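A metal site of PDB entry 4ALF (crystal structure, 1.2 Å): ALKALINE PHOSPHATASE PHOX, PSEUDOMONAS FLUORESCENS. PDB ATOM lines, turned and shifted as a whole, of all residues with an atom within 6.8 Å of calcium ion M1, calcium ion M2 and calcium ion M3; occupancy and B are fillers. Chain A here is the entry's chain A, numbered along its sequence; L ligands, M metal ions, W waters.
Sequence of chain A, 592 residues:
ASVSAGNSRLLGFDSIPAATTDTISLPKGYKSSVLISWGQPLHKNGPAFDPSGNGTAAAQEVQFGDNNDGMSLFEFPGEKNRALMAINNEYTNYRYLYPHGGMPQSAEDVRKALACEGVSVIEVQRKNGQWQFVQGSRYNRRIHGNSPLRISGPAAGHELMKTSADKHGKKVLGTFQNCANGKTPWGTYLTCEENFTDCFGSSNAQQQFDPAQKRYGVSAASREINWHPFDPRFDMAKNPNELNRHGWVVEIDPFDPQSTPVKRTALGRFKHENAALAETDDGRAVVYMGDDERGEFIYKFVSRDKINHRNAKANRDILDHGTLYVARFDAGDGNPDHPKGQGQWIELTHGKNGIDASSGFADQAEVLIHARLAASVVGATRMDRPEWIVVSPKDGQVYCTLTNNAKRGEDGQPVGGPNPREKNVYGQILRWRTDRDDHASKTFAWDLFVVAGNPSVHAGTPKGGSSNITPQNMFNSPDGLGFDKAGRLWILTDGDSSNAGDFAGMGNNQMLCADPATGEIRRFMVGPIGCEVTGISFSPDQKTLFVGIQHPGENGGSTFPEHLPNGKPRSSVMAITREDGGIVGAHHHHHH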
ATOM      1  N   ASP A  69       4.362   9.002   1.832  1.00  0.00           N
ATOM      2  CA  ASP A  69       3.840   9.173   3.181  1.00  0.00           C
ATOM      3  C   ASP A  69       2.722  10.207   3.131  1.00  0.00           C
ATOM      4  O   ASP A  69       1.768  10.028   2.361  1.00  0.00           O
ATOM      5  CB  ASP A  69       5.021   9.513   4.131  1.00  0.00           C
ATOM      6  CG  ASP A  69       4.766   9.153   5.578  1.00  0.00           C
ATOM      7  OD1 ASP A  69       3.592   9.094   5.998  1.00  0.00           O
ATOM      8  OD2 ASP A  69       5.778   8.960   6.277  1.00  0.00           O
ATOM      9  N   GLU A  90       9.402   9.906   2.487  1.00  0.00           N
ATOM     10  CA  GLU A  90      10.005  10.007   3.808  1.00  0.00           C
ATOM     11  C   GLU A  90      11.447   9.511   3.914  1.00  0.00           C
ATOM     12  O   GLU A  90      12.298  10.142   4.573  1.00  0.00           O
ATOM     13  CB  GLU A  90       9.133   9.290   4.865  1.00  0.00           C
ATOM     14  CG  GLU A  90       9.591   9.588   6.290  1.00  0.00           C
ATOM     15  CD  GLU A  90       8.784   8.855   7.320  1.00  0.00           C
ATOM     16  OE1 GLU A  90       8.493   7.645   7.102  1.00  0.00           O
ATOM     17  OE2 GLU A  90       8.511   9.462   8.403  1.00  0.00           O
ATOM     18  N   TYR A  91      11.724   8.344   3.327  1.00  0.00           N
ATOM     19  CA  TYR A  91      13.036   7.722   3.474  1.00  0.00           C
ATOM     20  C   TYR A  91      13.217   6.720   2.364  1.00  0.00           C
ATOM     21  O   TYR A  91      12.374   6.664   1.459  1.00  0.00           O
ATOM     22  CB  TYR A  91      13.247   7.124   4.883  1.00  0.00           C
ATOM     23  CG  TYR A  91      12.423   5.933   5.311  1.00  0.00           C
ATOM     24  CD1 TYR A  91      11.106   6.071   5.672  1.00  0.00           C
ATOM     25  CD2 TYR A  91      13.006   4.670   5.479  1.00  0.00           C
ATOM     26  CE1 TYR A  91      10.359   5.022   6.153  1.00  0.00           C
ATOM     27  CE2 TYR A  91      12.274   3.607   5.974  1.00  0.00           C
ATOM     28  CZ  TYR A  91      10.936   3.753   6.307  1.00  0.00           C
ATOM     29  OH  TYR A  91      10.180   2.718   6.820  1.00  0.00           O
ATOM     30  N   CYS A 179       7.626  13.396   6.626  1.00  0.00           N
ATOM     31  CA  CYS A 179       6.695  12.452   7.207  1.00  0.00           C
ATOM     32  C   CYS A 179       5.286  12.758   6.779  1.00  0.00           C
ATOM     33  O   CYS A 179       4.873  12.264   5.724  1.00  0.00           O
ATOM     34  CB  CYS A 179       6.882  12.465   8.719  1.00  0.00           C
ATOM     35  SG  CYS A 179       5.843  11.297   9.596  1.00  0.00           S
ATOM     36  N   ALA A 180       4.560  13.575   7.523  1.00  0.00           N
ATOM     37  CA  ALA A 180       3.214  13.915   7.087  1.00  0.00           C
ATOM     38  C   ALA A 180       3.028  15.410   6.849  1.00  0.00           C
ATOM     39  O   ALA A 180       4.004  16.119   6.580  1.00  0.00           O
ATOM     40  CB  ALA A 180       2.176  13.243   7.986  1.00  0.00           C
ATOM     41  N   GLU A 194      10.574  14.912  10.232  1.00  0.00           N
ATOM     42  CA  GLU A 194      10.451  14.078  11.438  1.00  0.00           C
ATOM     43  C   GLU A 194      11.805  13.542  11.887  1.00  0.00           C
ATOM     44  O   GLU A 194      12.465  14.190  12.699  1.00  0.00           O
ATOM     45  CB  GLU A 194       9.392  12.990  11.272  1.00  0.00           C
ATOM     46  CG  GLU A 194       9.112  12.188  12.510  1.00  0.00           C
ATOM     47  CD  GLU A 194       8.365  10.905  12.204  1.00  0.00           C
ATOM     48  OE1 GLU A 194       8.458  10.400  11.043  1.00  0.00           O
ATOM     49  OE2 GLU A 194       7.720  10.381  13.123  1.00  0.00           O
ATOM     50  N   GLU A 273       5.435  15.285  12.964  1.00  0.00           N
ATOM     51  CA  GLU A 273       4.661  14.283  12.245  1.00  0.00           C
ATOM     52  C   GLU A 273       3.773  14.965  11.182  1.00  0.00           C
ATOM     53  O   GLU A 273       4.065  14.878   9.994  1.00  0.00           O
ATOM     54  CB  GLU A 273       3.850  13.399  13.187  1.00  0.00           C
ATOM     55  CG  GLU A 273       3.129  12.312  12.402  1.00  0.00           C
ATOM     56  CD  GLU A 273       3.802  10.954  12.426  1.00  0.00           C
ATOM     57  OE1 GLU A 273       4.766  10.764  13.224  1.00  0.00           O
ATOM     58  OE2 GLU A 273       3.353  10.094  11.625  1.00  0.00           O
ATOM     59  N   ASP A 292       6.864  13.184  17.298  1.00  0.00           N
ATOM     60  CA  ASP A 292       6.831  11.733  17.441  1.00  0.00           C
ATOM     61  C   ASP A 292       8.117  11.199  17.977  1.00  0.00           C
ATOM     62  O   ASP A 292       9.033  10.865  17.256  1.00  0.00           O
ATOM     63  CB  ASP A 292       6.460  11.023  16.151  1.00  0.00           C
ATOM     64  CG  ASP A 292       6.454   9.519  16.319  1.00  0.00           C
ATOM     65  OD1 ASP A 292       6.549   9.039  17.471  1.00  0.00           O
ATOM     66  OD2 ASP A 292       6.338   8.809  15.288  1.00  0.00           O
ATOM     67  N   ARG A 385       4.103   8.917  21.983  1.00  0.00           N
ATOM     68  CA  ARG A 385       4.395   9.036  20.544  1.00  0.00           C
ATOM     69  C   ARG A 385       3.257   9.642  19.759  1.00  0.00           C
ATOM     70  O   ARG A 385       2.567   8.952  18.971  1.00  0.00           O
ATOM     71  CB  ARG A 385       4.777   7.685  19.945  1.00  0.00           C
ATOM     72  CG  ARG A 385       6.111   7.164  20.416  1.00  0.00           C
ATOM     73  CD  ARG A 385       6.500   5.957  19.611  1.00  0.00           C
ATOM     74  NE  ARG A 385       6.657   6.353  18.216  1.00  0.00           N
ATOM     75  CZ  ARG A 385       6.734   5.502  17.192  1.00  0.00           C
ATOM     76  NH1 ARG A 385       6.725   4.197  17.383  1.00  0.00           N
ATOM     77  NH2 ARG A 385       6.831   5.990  15.971  1.00  0.00           N
ATOM     78  N   GLU A 387       1.496  10.996  16.802  1.00  0.00           N
ATOM     79  CA  GLU A 387       1.707  10.997  15.347  1.00  0.00           C
ATOM     80  C   GLU A 387       0.666  11.959  14.739  1.00  0.00           C
ATOM     81  O   GLU A 387       0.690  13.155  15.040  1.00  0.00           O
ATOM     82  CB  GLU A 387       1.770   9.566  14.775  1.00  0.00           C
ATOM     83  CG  GLU A 387       3.045   8.875  15.209  1.00  0.00           C
ATOM     84  CD  GLU A 387       3.439   7.697  14.362  1.00  0.00           C
ATOM     85  OE1 GLU A 387       2.816   6.641  14.540  1.00  0.00           O
ATOM     86  OE2 GLU A 387       4.365   7.773  13.520  1.00  0.00           O
ATOM     87  N   TRP A 388      -0.243  11.523  13.885  1.00  0.00           N
ATOM     88  CA  TRP A 388      -1.077  12.484  13.190  1.00  0.00           C
ATOM     89  C   TRP A 388      -2.160  13.092  14.038  1.00  0.00           C
ATOM     90  O   TRP A 388      -2.729  12.424  14.901  1.00  0.00           O
ATOM     91  CB  TRP A 388      -1.791  11.904  11.981  1.00  0.00           C
ATOM     92  CG  TRP A 388      -0.898  11.410  10.866  1.00  0.00           C
ATOM     93  CD1 TRP A 388       0.286  10.716  10.969  1.00  0.00           C
ATOM     94  CD2 TRP A 388      -1.190  11.466   9.448  1.00  0.00           C
ATOM     95  NE1 TRP A 388       0.775  10.368   9.718  1.00  0.00           N
ATOM     96  CE2 TRP A 388      -0.096  10.760   8.786  1.00  0.00           C
ATOM     97  CE3 TRP A 388      -2.211  11.986   8.686  1.00  0.00           C
ATOM     98  CZ2 TRP A 388      -0.049  10.625   7.404  1.00  0.00           C
ATOM     99  CZ3 TRP A 388      -2.169  11.806   7.312  1.00  0.00           C
ATOM    100  CH2 TRP A 388      -1.115  11.159   6.688  1.00  0.00           C
ATOM    101  N   THR A 403       0.820   6.425  19.181  1.00  0.00           N
ATOM    102  CA  THR A 403       0.920   5.159  18.435  1.00  0.00           C
ATOM    103  C   THR A 403       1.273   3.954  19.294  1.00  0.00           C
ATOM    104  O   THR A 403       0.737   2.868  19.098  1.00  0.00           O
ATOM    105  CB  THR A 403       1.813   5.307  17.184  1.00  0.00           C
ATOM    106  OG1 THR A 403       1.535   4.237  16.281  1.00  0.00           O
ATOM    107  CG2 THR A 403       3.277   5.405  17.495  1.00  0.00           C
ATOM    108  N   ASN A 404       2.166   4.167  20.251  1.00  0.00           N
ATOM    109  CA  ASN A 404       2.622   3.185  21.220  1.00  0.00           C
ATOM    110  C   ASN A 404       3.692   3.843  22.086  1.00  0.00           C
ATOM    111  O   ASN A 404       4.125   4.977  21.819  1.00  0.00           O
ATOM    112  CB  ASN A 404       3.121   1.888  20.562  1.00  0.00           C
ATOM    113  CG  ASN A 404       4.160   2.122  19.490  1.00  0.00           C
ATOM    114  OD1 ASN A 404       5.218   2.710  19.724  1.00  0.00           O
ATOM    115  ND2 ASN A 404       3.873   1.650  18.251  1.00  0.00           N
ATOM    116  N   SER A 477      -1.090   0.235  16.782  1.00  0.00           N
ATOM    117  CA  SER A 477      -0.246   1.331  16.320  1.00  0.00           C
ATOM    118  C   SER A 477      -0.936   2.209  15.298  1.00  0.00           C
ATOM    119  O   SER A 477      -0.394   2.422  14.206  1.00  0.00           O
ATOM    120  CB  SER A 477       1.107   0.821  15.809  1.00  0.00           C
ATOM    121  OG  SER A 477       1.778   0.028  16.801  1.00  0.00           O
ATOM    122  N   PRO A 478      -2.099   2.776  15.618  1.00  0.00           N
ATOM    123  CA  PRO A 478      -2.681   3.771  14.736  1.00  0.00           C
ATOM    124  C   PRO A 478      -1.679   4.932  14.578  1.00  0.00           C
ATOM    125  O   PRO A 478      -0.940   5.242  15.524  1.00  0.00           O
ATOM    126  CB  PRO A 478      -3.924   4.204  15.518  1.00  0.00           C
ATOM    127  CG  PRO A 478      -3.548   4.031  16.965  1.00  0.00           C
ATOM    128  CD  PRO A 478      -2.684   2.802  16.968  1.00  0.00           C
ATOM    129  N   ASP A 479      -1.621   5.508  13.389  1.00  0.00           N
ATOM    130  CA  ASP A 479      -0.580   6.455  13.011  1.00  0.00           C
ATOM    131  C   ASP A 479      -1.284   7.565  12.218  1.00  0.00           C
ATOM    132  O   ASP A 479      -1.657   8.599  12.781  1.00  0.00           O
ATOM    133  CB  ASP A 479       0.531   5.674  12.280  1.00  0.00           C
ATOM    134  CG  ASP A 479       1.714   6.525  11.776  1.00  0.00           C
ATOM    135  OD1 ASP A 479       1.538   7.723  11.514  1.00  0.00           O
ATOM    136  OD2 ASP A 479       2.798   5.937  11.613  1.00  0.00           O
ATOM    137  N   GLY A 480      -1.553   7.309  10.953  1.00  0.00           N
ATOM    138  CA  GLY A 480      -2.280   8.255  10.159  1.00  0.00           C
ATOM    139  C   GLY A 480      -3.746   8.405  10.469  1.00  0.00           C
ATOM    140  O   GLY A 480      -4.376   7.475  10.952  1.00  0.00           O
ATOM    141  N   THR A 493      -2.831   2.379   9.933  1.00  0.00           N
ATOM    142  CA  THR A 493      -1.939   1.775  10.914  1.00  0.00           C
ATOM    143  C   THR A 493      -0.500   1.561  10.441  1.00  0.00           C
ATOM    144  O   THR A 493      -0.207   1.266   9.281  1.00  0.00           O
ATOM    145  CB  THR A 493      -2.498   0.447  11.518  1.00  0.00           C
ATOM    146  OG1 THR A 493      -2.326  -0.672  10.631  1.00  0.00           O
ATOM    147  CG2 THR A 493      -3.976   0.596  11.841  1.00  0.00           C
ATOM    148  N   ASP A 494       0.402   1.638  11.399  1.00  0.00           N
ATOM    149  CA  ASP A 494       1.825   1.415  11.213  1.00  0.00           C
ATOM    150  C   ASP A 494       2.327   0.617  12.412  1.00  0.00           C
ATOM    151  O   ASP A 494       3.074   1.115  13.246  1.00  0.00           O
ATOM    152  CB  ASP A 494       2.605   2.730  11.127  1.00  0.00           C
ATOM    153  CG  ASP A 494       4.092   2.539  11.082  1.00  0.00           C
ATOM    154  OD1 ASP A 494       4.550   1.459  10.658  1.00  0.00           O
ATOM    155  OD2 ASP A 494       4.862   3.447  11.480  1.00  0.00           O
ATOM    156  N   GLY A 495       1.922  -0.631  12.495  1.00  0.00           N
ATOM    157  CA  GLY A 495       2.202  -1.451  13.641  1.00  0.00           C
ATOM    158  C   GLY A 495       2.889  -2.724  13.273  1.00  0.00           C
ATOM    159  O   GLY A 495       3.360  -2.938  12.159  1.00  0.00           O
ATOM    160  N   GLU A 532       3.505  -0.256   5.646  1.00  0.00           N
ATOM    161  CA  GLU A 532       2.560   0.440   6.500  1.00  0.00           C
ATOM    162  C   GLU A 532       1.616   1.188   5.573  1.00  0.00           C
ATOM    163  O   GLU A 532       1.936   1.466   4.410  1.00  0.00           O
ATOM    164  CB  GLU A 532       3.232   1.370   7.522  1.00  0.00           C
ATOM    165  CG  GLU A 532       3.989   2.545   6.927  1.00  0.00           C
ATOM    166  CD  GLU A 532       4.853   3.217   7.981  1.00  0.00           C
ATOM    167  OE1 GLU A 532       5.934   2.694   8.262  1.00  0.00           O
ATOM    168  OE2 GLU A 532       4.399   4.233   8.552  1.00  0.00           O
ATOM    169  N   THR A 534      -0.249   4.646   4.955  1.00  0.00           N
ATOM    170  CA  THR A 534       0.044   6.024   5.375  1.00  0.00           C
ATOM    171  C   THR A 534      -0.234   6.952   4.221  1.00  0.00           C
ATOM    172  O   THR A 534      -0.036   6.589   3.077  1.00  0.00           O
ATOM    173  CB  THR A 534       1.485   6.101   5.907  1.00  0.00           C
ATOM    174  OG1 THR A 534       1.681   7.382   6.511  1.00  0.00           O
ATOM    175  CG2 THR A 534       2.523   5.806   4.828  1.00  0.00           C
ATOM    176  N   GLN A 550       3.442   2.226   1.993  1.00  0.00           N
ATOM    177  CA  GLN A 550       4.813   2.618   2.169  1.00  0.00           C
ATOM    178  C   GLN A 550       5.674   1.384   2.506  1.00  0.00           C
ATOM    179  O   GLN A 550       5.255   0.525   3.280  1.00  0.00           O
ATOM    180  CB  GLN A 550       4.938   3.657   3.311  1.00  0.00           C
ATOM    181  CG  GLN A 550       6.302   4.327   3.382  1.00  0.00           C
ATOM    182  CD  GLN A 550       6.478   5.094   4.674  1.00  0.00           C
ATOM    183  OE1 GLN A 550       6.271   4.552   5.756  1.00  0.00           O
ATOM    184  NE2 GLN A 550       6.809   6.382   4.552  1.00  0.00           N
ATOM    185  N   HIS A 551       6.850   1.320   1.875  1.00  0.00           N
ATOM    186  CA  HIS A 551       7.854   0.253   2.053  1.00  0.00           C
ATOM    187  C   HIS A 551       7.296  -1.145   2.014  1.00  0.00           C
ATOM    188  O   HIS A 551       7.642  -1.966   2.865  1.00  0.00           O
ATOM    189  CB  HIS A 551       8.746   0.467   3.313  1.00  0.00           C
ATOM    190  CG  HIS A 551       8.010   0.507   4.626  1.00  0.00           C
ATOM    191  ND1 HIS A 551       7.480  -0.583   5.217  1.00  0.00           N
ATOM    192  CD2 HIS A 551       7.782   1.563   5.469  1.00  0.00           C
ATOM    193  CE1 HIS A 551       6.914  -0.221   6.367  1.00  0.00           C
ATOM    194  NE2 HIS A 551       7.079   1.087   6.513  1.00  0.00           N
HETATM  195  P1  LIG L   1       7.220   6.574  11.651  1.00  0.00           P
HETATM  196  O1  LIG L   1       5.791   6.219  11.187  1.00  0.00           O
HETATM  197  O2  LIG L   1       7.972   7.425  10.613  1.00  0.00           O
HETATM  198  O3  LIG L   1       7.159   7.159  13.053  1.00  0.00           O
HETATM  199  O4  LIG L   1       7.946   5.240  11.696  1.00  0.00           O
HETATM  200 FE1  LG2 L   2       7.191   9.202   9.914  1.00  0.00          FE
HETATM  201 FE2  LG2 L   2       6.050   9.032  13.318  1.00  0.00          FE
HETATM  202  O1  LG2 L   2       5.843   9.001  11.390  1.00  0.00           O
HETATM  203 CA    CA M   1       4.480   5.308  13.036  1.00  0.00          CA
HETATM  204 CA    CA M   2       3.872   7.918  10.639  1.00  0.00          CA
HETATM  205 CA    CA M   3       6.687   4.080  10.042  1.00  0.00          CA
HETATM  206  O   HOH W   1       5.723   7.997   8.703  1.00  0.00           O
HETATM  207  O   HOH W   2       3.274   9.492   8.773  1.00  0.00           O
HETATM  208  O   HOH W   3       6.578   4.170  13.840  1.00  0.00           O
HETATM  209  O   HOH W   4       2.903   6.487   8.826  1.00  0.00           O
HETATM  210  O   HOH W   5       7.315   1.890  11.105  1.00  0.00           O
HETATM  211  O   HOH W   6       8.979   3.431   9.247  1.00  0.00           O
HETATM  212  O   HOH W   7       3.411   3.695  14.341  1.00  0.00           O
HETATM  213  O   HOH W   8       7.083   5.533   8.212  1.00  0.00           O
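OE1 of Glu 273 is bound to FE2 of LG2 L2 (2.2 Å). FE2 of LG2 L2 is bound by OE2 of Glu 387 (2.1 Å). An iron atom (FE1) of LG2 L2 is bound by the side-chain sulfur (SG) of Cys 179, at 2.5 Å. OD2 of Asp 292 is bound to FE2 of LG2 L2, 2.0 Å away. The side-chain carboxylate (OE2) of Glu 90 binds an iron atom (FE1) of LG2 L2, at 2.0 Å. An iron atom (FE1) of LG2 L2 is bound by the side-chain carboxylate (OE1) of Glu 194.
Calcium ion M1 is bound by the side-chain carboxylate (OD2) of Asp 479 (2.3 Å), water W7 (2.3 Å), an oxygen (O1) of LIG L1 (2.4 Å), the side-chain carboxylate (OD2) of Asp 494 (2.5 Å), the side-chain carboxylate (OE2) of Glu 387 (2.5 Å), water W3 (2.5 Å) and the side-chain carboxylate (OE1) of Glu 387 (2.6 Å).
Calcium ion M3 is bound by water W8 (2.4 Å), OE1 of Glu 532 (2.4 Å), O4 of LIG L1 (2.4 Å), OD2 of Asp 494 (2.4 Å), water W6 (2.5 Å), water W5 (2.5 Å), O1 of LIG L1 (2.6 Å) and OE2 of Glu 532 (2.7 Å). Calcium ion M3 has eight donor atoms within binding distance.
Calcium ion M2 is bound by an oxygen (O1) of LG2 L2 (2.4 Å), the side-chain carboxylate (OE2) of Glu 273 (2.4 Å), the side-chain carboxylate (OD2) of Asp 479 (2.5 Å), the side-chain carboxylate (OD1) of Asp 479 (2.5 Å), water W4 (2.5 Å), water W2 (2.5 Å), an oxygen (O1) of LIG L1 (2.6 Å) and water W1 (2.7 Å). Slightly farther from calcium ion M2 lies the side-chain carboxylate (OE2) of Glu 387 (2.9 Å).
The backbone carbonyl oxygen (O) of Asp 479 lies close to the backbone NH (N) of Trp 388 (3.4 Å). The backbone NH (N) of Gln 550 sits at hydrogen-bond distance from the backbone carbonyl oxygen (O) of Glu 532, 2.9 Å away. O of Ser 477 lies within hydrogen-bond range of N of Asp 494 (3.0 Å). The indole nitrogen (NE1) of Trp 388 lies close to the side-chain carboxylate (OE2) of Glu 273. The side-chain carboxylate of Glu 387 sits close to the side-chain hydroxyl of Thr 403. The backbone NH (N) of Thr 403 sits at hydrogen-bond distance from the backbone carbonyl oxygen (O) of Arg 385 (3.1 Å). The guanidinium group (NE) of Arg 385 lies within salt-bridge range of the side-chain carboxylate (OD1) of Asp 292, at 2.8 Å. OD1 of Asn 404 is in hydrogen-bond range of NH1 of Arg 385.
Merely in contact with calcium ion M1: Arg 385 (3.8 Å). Of the 24 residues printed, 4 come within 4 Å of calcium ion M1. The nearest printed residue that does not touch calcium ion M1 is Thr 403 (4.5 Å).
Water W7 lies within hydrogen-bond range of the side-chain hydroxyl (OG1) of Thr 403 and the backbone carbonyl oxygen (O) of Asp 494. Water W2 lies within hydrogen-bond range of NE1 of Trp 388 (2.8 Å), OD1 of Asp 69 (2.8 Å) and OG1 of Thr 534 (3.5 Å). Water W1 lies within hydrogen-bond range of OD2 of Asp 69 and OE1 of Glu 90. Water W8 bridges OE1 of Gln 550 (2.8 Å) and OE1 of Glu 90 (2.8 Å).
Of the 24 residues printed, 2 come within 4 Å of calcium ion M3. The nearest printed residue that does not touch calcium ion M3 is Gln 550 (4.3 Å).
Within 4 Å of calcium ion M2: Glu 273, Glu 387 and Asp 479. The nearest printed residue that does not touch calcium ion M2 is Cys 179 (4.05 Å).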
